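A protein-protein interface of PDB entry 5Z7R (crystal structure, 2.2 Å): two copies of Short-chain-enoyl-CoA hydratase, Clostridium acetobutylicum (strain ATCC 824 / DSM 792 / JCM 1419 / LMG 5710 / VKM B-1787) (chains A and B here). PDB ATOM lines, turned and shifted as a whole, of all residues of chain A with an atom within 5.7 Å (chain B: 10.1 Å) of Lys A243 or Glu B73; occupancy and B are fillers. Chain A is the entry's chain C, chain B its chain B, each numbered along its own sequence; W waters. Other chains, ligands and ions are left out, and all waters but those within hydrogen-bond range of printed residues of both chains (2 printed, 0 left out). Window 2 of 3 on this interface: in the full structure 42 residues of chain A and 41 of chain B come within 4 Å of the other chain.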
ATOM      1  N   THR A 239     -31.589 -26.706 -27.267  1.00  0.00           N
ATOM      2  CA  THR A 239     -30.917 -27.392 -26.157  1.00  0.00           C
ATOM      3  C   THR A 239     -30.073 -26.470 -25.273  1.00  0.00           C
ATOM      4  O   THR A 239     -29.420 -25.576 -25.753  1.00  0.00           O
ATOM      5  CB  THR A 239     -29.991 -28.580 -26.658  1.00  0.00           C
ATOM      6  OG1 THR A 239     -28.884 -28.081 -27.414  1.00  0.00           O
ATOM      7  CG2 THR A 239     -30.751 -29.551 -27.515  1.00  0.00           C
ATOM      8  N   GLU A 240     -30.053 -26.784 -23.984  1.00  0.00           N
ATOM      9  CA  GLU A 240     -29.102 -26.200 -23.026  1.00  0.00           C
ATOM     10  C   GLU A 240     -27.663 -26.399 -23.425  1.00  0.00           C
ATOM     11  O   GLU A 240     -26.871 -25.459 -23.319  1.00  0.00           O
ATOM     12  CB  GLU A 240     -29.243 -26.835 -21.625  1.00  0.00           C
ATOM     13  CG  GLU A 240     -30.555 -26.548 -20.928  1.00  0.00           C
ATOM     14  CD  GLU A 240     -30.812 -25.069 -20.820  1.00  0.00           C
ATOM     15  OE1 GLU A 240     -29.918 -24.339 -20.306  1.00  0.00           O
ATOM     16  OE2 GLU A 240     -31.902 -24.652 -21.270  1.00  0.00           O
ATOM     17  N   ASP A 241     -27.304 -27.625 -23.821  1.00  0.00           N
ATOM     18  CA  ASP A 241     -25.907 -27.892 -24.131  1.00  0.00           C
ATOM     19  C   ASP A 241     -25.422 -26.845 -25.115  1.00  0.00           C
ATOM     20  O   ASP A 241     -24.300 -26.404 -25.019  1.00  0.00           O
ATOM     21  CB  ASP A 241     -25.670 -29.282 -24.725  1.00  0.00           C
ATOM     22  CG  ASP A 241     -25.423 -30.367 -23.677  1.00  0.00           C
ATOM     23  OD1 ASP A 241     -25.980 -30.332 -22.573  1.00  0.00           O
ATOM     24  OD2 ASP A 241     -24.683 -31.316 -23.989  1.00  0.00           O
ATOM     25  N   GLN A 242     -26.258 -26.431 -26.057  1.00  0.00           N
ATOM     26  CA  GLN A 242     -25.818 -25.432 -27.041  1.00  0.00           C
ATOM     27  C   GLN A 242     -25.596 -24.047 -26.430  1.00  0.00           C
ATOM     28  O   GLN A 242     -24.560 -23.414 -26.630  1.00  0.00           O
ATOM     29  CB  GLN A 242     -26.820 -25.370 -28.218  1.00  0.00           C
ATOM     30  CG  GLN A 242     -26.593 -24.203 -29.168  1.00  0.00           C
ATOM     31  CD  GLN A 242     -27.319 -22.921 -28.753  1.00  0.00           C
ATOM     32  OE1 GLN A 242     -28.476 -22.952 -28.364  1.00  0.00           O
ATOM     33  NE2 GLN A 242     -26.642 -21.798 -28.882  1.00  0.00           N
ATOM     34  N   LYS A 243     -26.607 -23.584 -25.728  1.00  0.00           N
ATOM     35  CA  LYS A 243     -26.549 -22.362 -24.920  1.00  0.00           C
ATOM     36  C   LYS A 243     -25.356 -22.396 -23.977  1.00  0.00           C
ATOM     37  O   LYS A 243     -24.527 -21.498 -23.984  1.00  0.00           O
ATOM     38  CB  LYS A 243     -27.870 -22.235 -24.146  1.00  0.00           C
ATOM     39  CG  LYS A 243     -27.928 -21.216 -23.019  1.00  0.00           C
ATOM     40  CD  LYS A 243     -27.806 -19.774 -23.499  1.00  0.00           C
ATOM     41  CE  LYS A 243     -28.145 -18.785 -22.379  1.00  0.00           C
ATOM     42  NZ  LYS A 243     -27.553 -17.426 -22.605  1.00  0.00           N
ATOM     43  N   ASP A 244     -25.230 -23.478 -23.227  1.00  0.00           N
ATOM     44  CA  ASP A 244     -24.117 -23.635 -22.272  1.00  0.00           C
ATOM     45  C   ASP A 244     -22.738 -23.762 -22.870  1.00  0.00           C
ATOM     46  O   ASP A 244     -21.808 -23.120 -22.398  1.00  0.00           O
ATOM     47  CB  ASP A 244     -24.383 -24.823 -21.344  1.00  0.00           C
ATOM     48  CG  ASP A 244     -25.555 -24.577 -20.442  1.00  0.00           C
ATOM     49  OD1 ASP A 244     -26.022 -23.424 -20.428  1.00  0.00           O
ATOM     50  OD2 ASP A 244     -26.037 -25.511 -19.767  1.00  0.00           O
ATOM     51  N   ALA A 245     -22.586 -24.574 -23.908  1.00  0.00           N
ATOM     52  CA  ALA A 245     -21.262 -24.760 -24.512  1.00  0.00           C
ATOM     53  C   ALA A 245     -20.810 -23.489 -25.179  1.00  0.00           C
ATOM     54  O   ALA A 245     -19.634 -23.165 -25.146  1.00  0.00           O
ATOM     55  CB  ALA A 245     -21.259 -25.900 -25.525  1.00  0.00           C
ATOM     56  N   MET A 246     -21.731 -22.781 -25.823  1.00  0.00           N
ATOM     57  CA  MET A 246     -21.367 -21.516 -26.468  1.00  0.00           C
ATOM     58  C   MET A 246     -21.003 -20.446 -25.423  1.00  0.00           C
ATOM     59  O   MET A 246     -19.959 -19.810 -25.518  1.00  0.00           O
ATOM     60  CB  MET A 246     -22.490 -21.051 -27.385  1.00  0.00           C
ATOM     61  CG  MET A 246     -22.652 -21.955 -28.609  1.00  0.00           C
ATOM     62  SD  MET A 246     -23.465 -21.187 -30.024  1.00  0.00           S
ATOM     63  CE  MET A 246     -23.597 -22.622 -31.070  1.00  0.00           C
ATOM     64  N   THR A 247     -21.848 -20.279 -24.408  1.00  0.00           N
ATOM     65  CA  THR A 247     -21.555 -19.343 -23.327  1.00  0.00           C
ATOM     66  C   THR A 247     -20.155 -19.647 -22.788  1.00  0.00           C
ATOM     67  O   THR A 247     -19.242 -18.818 -22.877  1.00  0.00           O
ATOM     68  CB  THR A 247     -22.616 -19.428 -22.204  1.00  0.00           C
ATOM     69  OG1 THR A 247     -23.910 -19.094 -22.727  1.00  0.00           O
ATOM     70  CG2 THR A 247     -22.300 -18.450 -21.077  1.00  0.00           C
ATOM     71  N   ALA A 248     -19.980 -20.860 -22.284  1.00  0.00           N
ATOM     72  CA  ALA A 248     -18.671 -21.330 -21.844  1.00  0.00           C
ATOM     73  C   ALA A 248     -17.562 -20.949 -22.814  1.00  0.00           C
ATOM     74  O   ALA A 248     -16.532 -20.462 -22.404  1.00  0.00           O
ATOM     75  CB  ALA A 248     -18.689 -22.838 -21.641  1.00  0.00           C
ATOM     76  N   ASP B  67     -18.565 -16.607 -35.936  1.00  0.00           N
ATOM     77  CA  ASP B  67     -18.639 -15.910 -34.652  1.00  0.00           C
ATOM     78  C   ASP B  67     -19.715 -16.529 -33.778  1.00  0.00           C
ATOM     79  O   ASP B  67     -20.893 -16.528 -34.142  1.00  0.00           O
ATOM     80  CB  ASP B  67     -18.909 -14.409 -34.828  1.00  0.00           C
ATOM     81  CG  ASP B  67     -19.031 -13.687 -33.491  1.00  0.00           C
ATOM     82  OD1 ASP B  67     -17.993 -13.431 -32.847  1.00  0.00           O
ATOM     83  OD2 ASP B  67     -20.170 -13.409 -33.052  1.00  0.00           O
ATOM     84  N   ILE B  68     -19.315 -17.034 -32.617  1.00  0.00           N
ATOM     85  CA  ILE B  68     -20.242 -17.675 -31.701  1.00  0.00           C
ATOM     86  C   ILE B  68     -21.160 -16.712 -30.928  1.00  0.00           C
ATOM     87  O   ILE B  68     -22.305 -17.071 -30.620  1.00  0.00           O
ATOM     88  CB  ILE B  68     -19.482 -18.591 -30.740  1.00  0.00           C
ATOM     89  CG1 ILE B  68     -18.777 -19.689 -31.542  1.00  0.00           C
ATOM     90  CG2 ILE B  68     -20.429 -19.203 -29.713  1.00  0.00           C
ATOM     91  CD1 ILE B  68     -19.725 -20.523 -32.409  1.00  0.00           C
ATOM     92  N   SER B  69     -20.683 -15.506 -30.617  1.00  0.00           N
ATOM     93  CA  SER B  69     -21.548 -14.471 -29.991  1.00  0.00           C
ATOM     94  C   SER B  69     -22.827 -14.301 -30.788  1.00  0.00           C
ATOM     95  O   SER B  69     -23.918 -14.158 -30.230  1.00  0.00           O
ATOM     96  CB  SER B  69     -20.847 -13.102 -29.927  1.00  0.00           C
ATOM     97  OG  SER B  69     -19.434 -13.263 -29.929  1.00  0.00           O
ATOM     98  N   GLU B  70     -22.664 -14.313 -32.105  1.00  0.00           N
ATOM     99  CA  GLU B  70     -23.767 -14.170 -33.028  1.00  0.00           C
ATOM    100  C   GLU B  70     -24.764 -15.298 -32.895  1.00  0.00           C
ATOM    101  O   GLU B  70     -25.915 -15.088 -33.098  1.00  0.00           O
ATOM    102  CB  GLU B  70     -23.232 -14.146 -34.445  1.00  0.00           C
ATOM    103  CG  GLU B  70     -24.093 -13.385 -35.406  1.00  0.00           C
ATOM    104  CD  GLU B  70     -23.267 -12.796 -36.521  1.00  0.00           C
ATOM    105  OE1 GLU B  70     -23.370 -13.325 -37.634  1.00  0.00           O
ATOM    106  OE2 GLU B  70     -22.496 -11.833 -36.281  1.00  0.00           O
ATOM    107  N   MET B  71     -24.307 -16.486 -32.523  1.00  0.00           N
ATOM    108  CA  MET B  71     -25.125 -17.681 -32.578  1.00  0.00           C
ATOM    109  C   MET B  71     -25.765 -18.065 -31.242  1.00  0.00           C
ATOM    110  O   MET B  71     -26.832 -18.667 -31.218  1.00  0.00           O
ATOM    111  CB  MET B  71     -24.256 -18.834 -33.066  1.00  0.00           C
ATOM    112  CG  MET B  71     -23.692 -18.666 -34.475  1.00  0.00           C
ATOM    113  SD  MET B  71     -22.777 -20.118 -35.126  1.00  0.00           S
ATOM    114  CE  MET B  71     -24.018 -21.355 -34.852  1.00  0.00           C
ATOM    115  N   LYS B  72     -25.127 -17.688 -30.139  1.00  0.00           N
ATOM    116  CA  LYS B  72     -25.462 -18.182 -28.793  1.00  0.00           C
ATOM    117  C   LYS B  72     -26.913 -17.997 -28.372  1.00  0.00           C
ATOM    118  O   LYS B  72     -27.473 -18.817 -27.637  1.00  0.00           O
ATOM    119  CB  LYS B  72     -24.545 -17.501 -27.769  1.00  0.00           C
ATOM    120  CG  LYS B  72     -25.030 -17.617 -26.326  1.00  0.00           C
ATOM    121  CD  LYS B  72     -23.959 -17.156 -25.345  1.00  0.00           C
ATOM    122  CE  LYS B  72     -24.524 -16.411 -24.133  1.00  0.00           C
ATOM    123  NZ  LYS B  72     -24.519 -14.934 -24.345  1.00  0.00           N
ATOM    124  N   GLU B  73     -27.531 -16.917 -28.823  1.00  0.00           N
ATOM    125  CA  GLU B  73     -28.863 -16.567 -28.342  1.00  0.00           C
ATOM    126  C   GLU B  73     -29.969 -17.068 -29.270  1.00  0.00           C
ATOM    127  O   GLU B  73     -31.149 -17.026 -28.935  1.00  0.00           O
ATOM    128  CB  GLU B  73     -28.974 -15.042 -28.145  1.00  0.00           C
ATOM    129  CG  GLU B  73     -28.359 -14.507 -26.855  1.00  0.00           C
ATOM    130  CD  GLU B  73     -28.942 -15.173 -25.625  1.00  0.00           C
ATOM    131  OE1 GLU B  73     -30.124 -14.916 -25.269  1.00  0.00           O
ATOM    132  OE2 GLU B  73     -28.208 -15.969 -25.007  1.00  0.00           O
ATOM    133  N   MET B  74     -29.594 -17.581 -30.425  1.00  0.00           N
ATOM    134  CA  MET B  74     -30.608 -17.986 -31.391  1.00  0.00           C
ATOM    135  C   MET B  74     -31.478 -19.100 -30.819  1.00  0.00           C
ATOM    136  O   MET B  74     -31.018 -19.915 -30.023  1.00  0.00           O
ATOM    137  CB  MET B  74     -29.959 -18.456 -32.686  1.00  0.00           C
ATOM    138  CG  MET B  74     -29.038 -17.448 -33.322  1.00  0.00           C
ATOM    139  SD  MET B  74     -28.450 -18.025 -34.922  1.00  0.00           S
ATOM    140  CE  MET B  74     -28.241 -16.433 -35.723  1.00  0.00           C
ATOM    141  N   ASN B  75     -32.739 -19.103 -31.221  1.00  0.00           N
ATOM    142  CA  ASN B  75     -33.643 -20.222 -30.983  1.00  0.00           C
ATOM    143  C   ASN B  75     -33.639 -21.211 -32.176  1.00  0.00           C
ATOM    144  O   ASN B  75     -32.839 -21.053 -33.110  1.00  0.00           O
ATOM    145  CB  ASN B  75     -35.051 -19.708 -30.629  1.00  0.00           C
ATOM    146  CG  ASN B  75     -35.878 -19.256 -31.840  1.00  0.00           C
ATOM    147  OD1 ASN B  75     -35.360 -18.903 -32.901  1.00  0.00           O
ATOM    148  ND2 ASN B  75     -37.201 -19.244 -31.655  1.00  0.00           N
ATOM    149  N   THR B  76     -34.510 -22.217 -32.121  1.00  0.00           N
ATOM    150  CA  THR B  76     -34.527 -23.306 -33.118  1.00  0.00           C
ATOM    151  C   THR B  76     -34.728 -22.754 -34.524  1.00  0.00           C
ATOM    152  O   THR B  76     -33.945 -23.008 -35.429  1.00  0.00           O
ATOM    153  CB  THR B  76     -35.617 -24.329 -32.781  1.00  0.00           C
ATOM    154  OG1 THR B  76     -35.123 -25.200 -31.774  1.00  0.00           O
ATOM    155  CG2 THR B  76     -36.001 -25.174 -33.970  1.00  0.00           C
ATOM    156  N   ILE B  77     -35.756 -21.937 -34.659  1.00  0.00           N
ATOM    157  CA  ILE B  77     -36.159 -21.385 -35.927  1.00  0.00           C
ATOM    158  C   ILE B  77     -35.162 -20.359 -36.426  1.00  0.00           C
ATOM    159  O   ILE B  77     -34.964 -20.258 -37.623  1.00  0.00           O
ATOM    160  CB  ILE B  77     -37.588 -20.774 -35.820  1.00  0.00           C
ATOM    161  CG1 ILE B  77     -38.587 -21.844 -35.339  1.00  0.00           C
ATOM    162  CG2 ILE B  77     -38.041 -20.170 -37.148  1.00  0.00           C
ATOM    163  CD1 ILE B  77     -38.581 -23.149 -36.145  1.00  0.00           C
ATOM    164  N   GLU B  78     -34.520 -19.609 -35.543  1.00  0.00           N
ATOM    165  CA  GLU B  78     -33.483 -18.683 -36.001  1.00  0.00           C
ATOM    166  C   GLU B  78     -32.215 -19.434 -36.491  1.00  0.00           C
ATOM    167  O   GLU B  78     -31.579 -19.039 -37.490  1.00  0.00           O
ATOM    168  CB  GLU B  78     -33.120 -17.674 -34.911  1.00  0.00           C
ATOM    169  CG  GLU B  78     -34.219 -16.645 -34.575  1.00  0.00           C
ATOM    170  CD  GLU B  78     -34.100 -16.000 -33.170  1.00  0.00           C
ATOM    171  OE1 GLU B  78     -33.066 -16.124 -32.477  1.00  0.00           O
ATOM    172  OE2 GLU B  78     -35.068 -15.333 -32.756  1.00  0.00           O
ATOM    173  N   GLY B  79     -31.856 -20.519 -35.810  1.00  0.00           N
ATOM    174  CA  GLY B  79     -30.605 -21.166 -36.103  1.00  0.00           C
ATOM    175  C   GLY B  79     -30.726 -21.834 -37.459  1.00  0.00           C
ATOM    176  O   GLY B  79     -29.788 -21.840 -38.248  1.00  0.00           O
ATOM    177  N   PHE B  82     -30.284 -19.315 -39.990  1.00  0.00           N
ATOM    178  CA  PHE B  82     -28.876 -19.010 -40.051  1.00  0.00           C
ATOM    179  C   PHE B  82     -28.120 -20.130 -40.808  1.00  0.00           C
ATOM    180  O   PHE B  82     -27.220 -19.848 -41.602  1.00  0.00           O
ATOM    181  CB  PHE B  82     -28.332 -18.766 -38.640  1.00  0.00           C
ATOM    182  CG  PHE B  82     -26.883 -18.347 -38.624  1.00  0.00           C
ATOM    183  CD1 PHE B  82     -26.503 -17.093 -39.079  1.00  0.00           C
ATOM    184  CD2 PHE B  82     -25.883 -19.230 -38.188  1.00  0.00           C
ATOM    185  CE1 PHE B  82     -25.154 -16.698 -39.071  1.00  0.00           C
ATOM    186  CE2 PHE B  82     -24.547 -18.847 -38.172  1.00  0.00           C
ATOM    187  CZ  PHE B  82     -24.176 -17.583 -38.611  1.00  0.00           C
ATOM    188  N   GLU B 134     -17.806 -28.147 -34.125  1.00  0.00           N
ATOM    189  CA  GLU B 134     -19.186 -27.785 -33.805  1.00  0.00           C
ATOM    190  C   GLU B 134     -19.863 -28.650 -32.743  1.00  0.00           C
ATOM    191  O   GLU B 134     -20.705 -28.177 -31.995  1.00  0.00           O
ATOM    192  CB  GLU B 134     -20.080 -27.773 -35.069  1.00  0.00           C
ATOM    193  CG  GLU B 134     -19.812 -26.606 -36.023  1.00  0.00           C
ATOM    194  CD  GLU B 134     -18.760 -26.935 -37.020  1.00  0.00           C
ATOM    195  OE1 GLU B 134     -18.596 -26.205 -38.030  1.00  0.00           O
ATOM    196  OE2 GLU B 134     -18.094 -27.986 -36.803  1.00  0.00           O
ATOM    197  N   GLY B 136     -18.720 -29.986 -30.135  1.00  0.00           N
ATOM    198  CA  GLY B 136     -18.294 -29.578 -28.813  1.00  0.00           C
ATOM    199  C   GLY B 136     -18.959 -28.290 -28.356  1.00  0.00           C
ATOM    200  O   GLY B 136     -18.799 -27.887 -27.205  1.00  0.00           O
ATOM    201  N   LEU B 137     -19.645 -27.616 -29.284  1.00  0.00           N
ATOM    202  CA  LEU B 137     -20.328 -26.356 -29.020  1.00  0.00           C
ATOM    203  C   LEU B 137     -21.813 -26.598 -28.976  1.00  0.00           C
ATOM    204  O   LEU B 137     -22.586 -25.676 -28.818  1.00  0.00           O
ATOM    205  CB  LEU B 137     -19.986 -25.299 -30.058  1.00  0.00           C
ATOM    206  CG  LEU B 137     -18.686 -24.508 -29.909  1.00  0.00           C
ATOM    207  CD1 LEU B 137     -17.547 -25.340 -29.379  1.00  0.00           C
ATOM    208  CD2 LEU B 137     -18.280 -23.890 -31.242  1.00  0.00           C
ATOM    209  N   GLY B 138     -22.217 -27.850 -29.070  1.00  0.00           N
ATOM    210  CA  GLY B 138     -23.608 -28.200 -28.888  1.00  0.00           C
ATOM    211  C   GLY B 138     -24.409 -28.134 -30.167  1.00  0.00           C
ATOM    212  O   GLY B 138     -25.615 -28.193 -30.104  1.00  0.00           O
ATOM    213  N   ILE B 139     -23.734 -28.096 -31.309  1.00  0.00           N
ATOM    214  CA  ILE B 139     -24.397 -28.082 -32.630  1.00  0.00           C
ATOM    215  C   ILE B 139     -23.777 -29.031 -33.666  1.00  0.00           C
ATOM    216  O   ILE B 139     -22.646 -29.500 -33.528  1.00  0.00           O
ATOM    217  CB  ILE B 139     -24.363 -26.680 -33.263  1.00  0.00           C
ATOM    218  CG1 ILE B 139     -22.971 -26.076 -33.089  1.00  0.00           C
ATOM    219  CG2 ILE B 139     -25.464 -25.819 -32.648  1.00  0.00           C
ATOM    220  CD1 ILE B 139     -22.639 -24.888 -33.973  1.00  0.00           C
HETATM  221  O   HOH W   1     -26.699 -29.680 -28.198  1.00  0.00           O
HETATM  222  O   HOH W   2     -30.674 -21.051 -27.531  1.00  0.00           O
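Lys A243 touches just these residues of chain B: Lys B72 and Glu B73.
Of chain A, only Lys A243 comes within 4 Å of Glu B73.
No residue of chain B comes within 4 Å of Asp A244.
Thr A247 touches one residue of chain B.
Of the printed residues of chain A, Gly B136 touches Ala A245 (3.6 Å).
Printed residues of chain A within 4 Å of Ile B68: Met A246.
Of the printed residues of chain A, Gly B138 touches Gln A242 (3.6 Å).
Thr B76 touches none of the printed residues of chain A.
Phe B82 touches none of the printed residues of chain A.
The nearest residue of chain A that does not touch Glu B73 is Gln A242 (5.0 Å).
SD of Met A246 is in hydrogen-bond range of NE2 of Gln A242 (3.4 Å).
The side-chain amino group (NZ) of Lys B72 is in salt-bridge range of the side-chain carboxylate (OE2) of Glu B73 (3.9 Å).
OG1 of Thr A247 is in hydrogen-bond range of O of Lys A243.
OG1 of Thr A239 lies within hydrogen-bond range of N of Gln A242 (3.4 Å).
The backbone carbonyl oxygen (O) of Glu B134 is in hydrogen-bond range of the backbone NH (N) of Ile B139, at 3.1 Å.
Of the 10 printed residues of chain A, 5 touch a printed residue of chain B.
Hydrophobic or aromatic side chains of chain A that line the printed part of chain B: Ala A245 and Met A246.
Of the 19 printed residues of chain B, 8 touch a printed residue of chain A.
Hydrophobic or aromatic side chains of chain B within 4 Å of the printed part of chain A: Ile B68, Met B71 and Ile B139.
Among the printed residues, 15 pairs touch across the chains.
Met B71 touches Gln A242 (O to NE2, 3.9 Å).
Gln A242 touches Leu B137 (CA to O, 3.7 Å).
Gln A242 touches Gly B138 (CB to O, 3.6 Å).
CB of Ala A245 touches O of Gly B136, at 3.6 Å.
Leu B137 touches Ala A245.
Ile B68 touches Met A246 (CG2 to CB, 3.6 Å).
Met B71 touches Met A246 (CB to SD, 3.9 Å).
Lys B72 touches Met A246 (CA to SD, 3.8 Å).
Met A246 touches Ile B139.
Thr A247 touches Lys B72.
No position is printed for both chains.
Of the 15 pairs that touch across the chains among the printed residues, none has its exchanged pair printed and touching as well.
NZ of Lys A243 lies within salt-bridge range of OE2 of Glu B73, 2.9 Å away.
The side-chain amide nitrogen (NE2) of Gln A242 is in hydrogen-bond range of the backbone carbonyl oxygen (O) of Lys B72, at 3.3 Å.
Water W1 lies within hydrogen-bond range of O of Gly B138 (2.6 Å) and OG1 of Thr A239 (2.8 Å).
Water W2 lies within hydrogen-bond range of O of Met B74 (2.8 Å) and OE1 of Gln A242 (3.0 Å).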
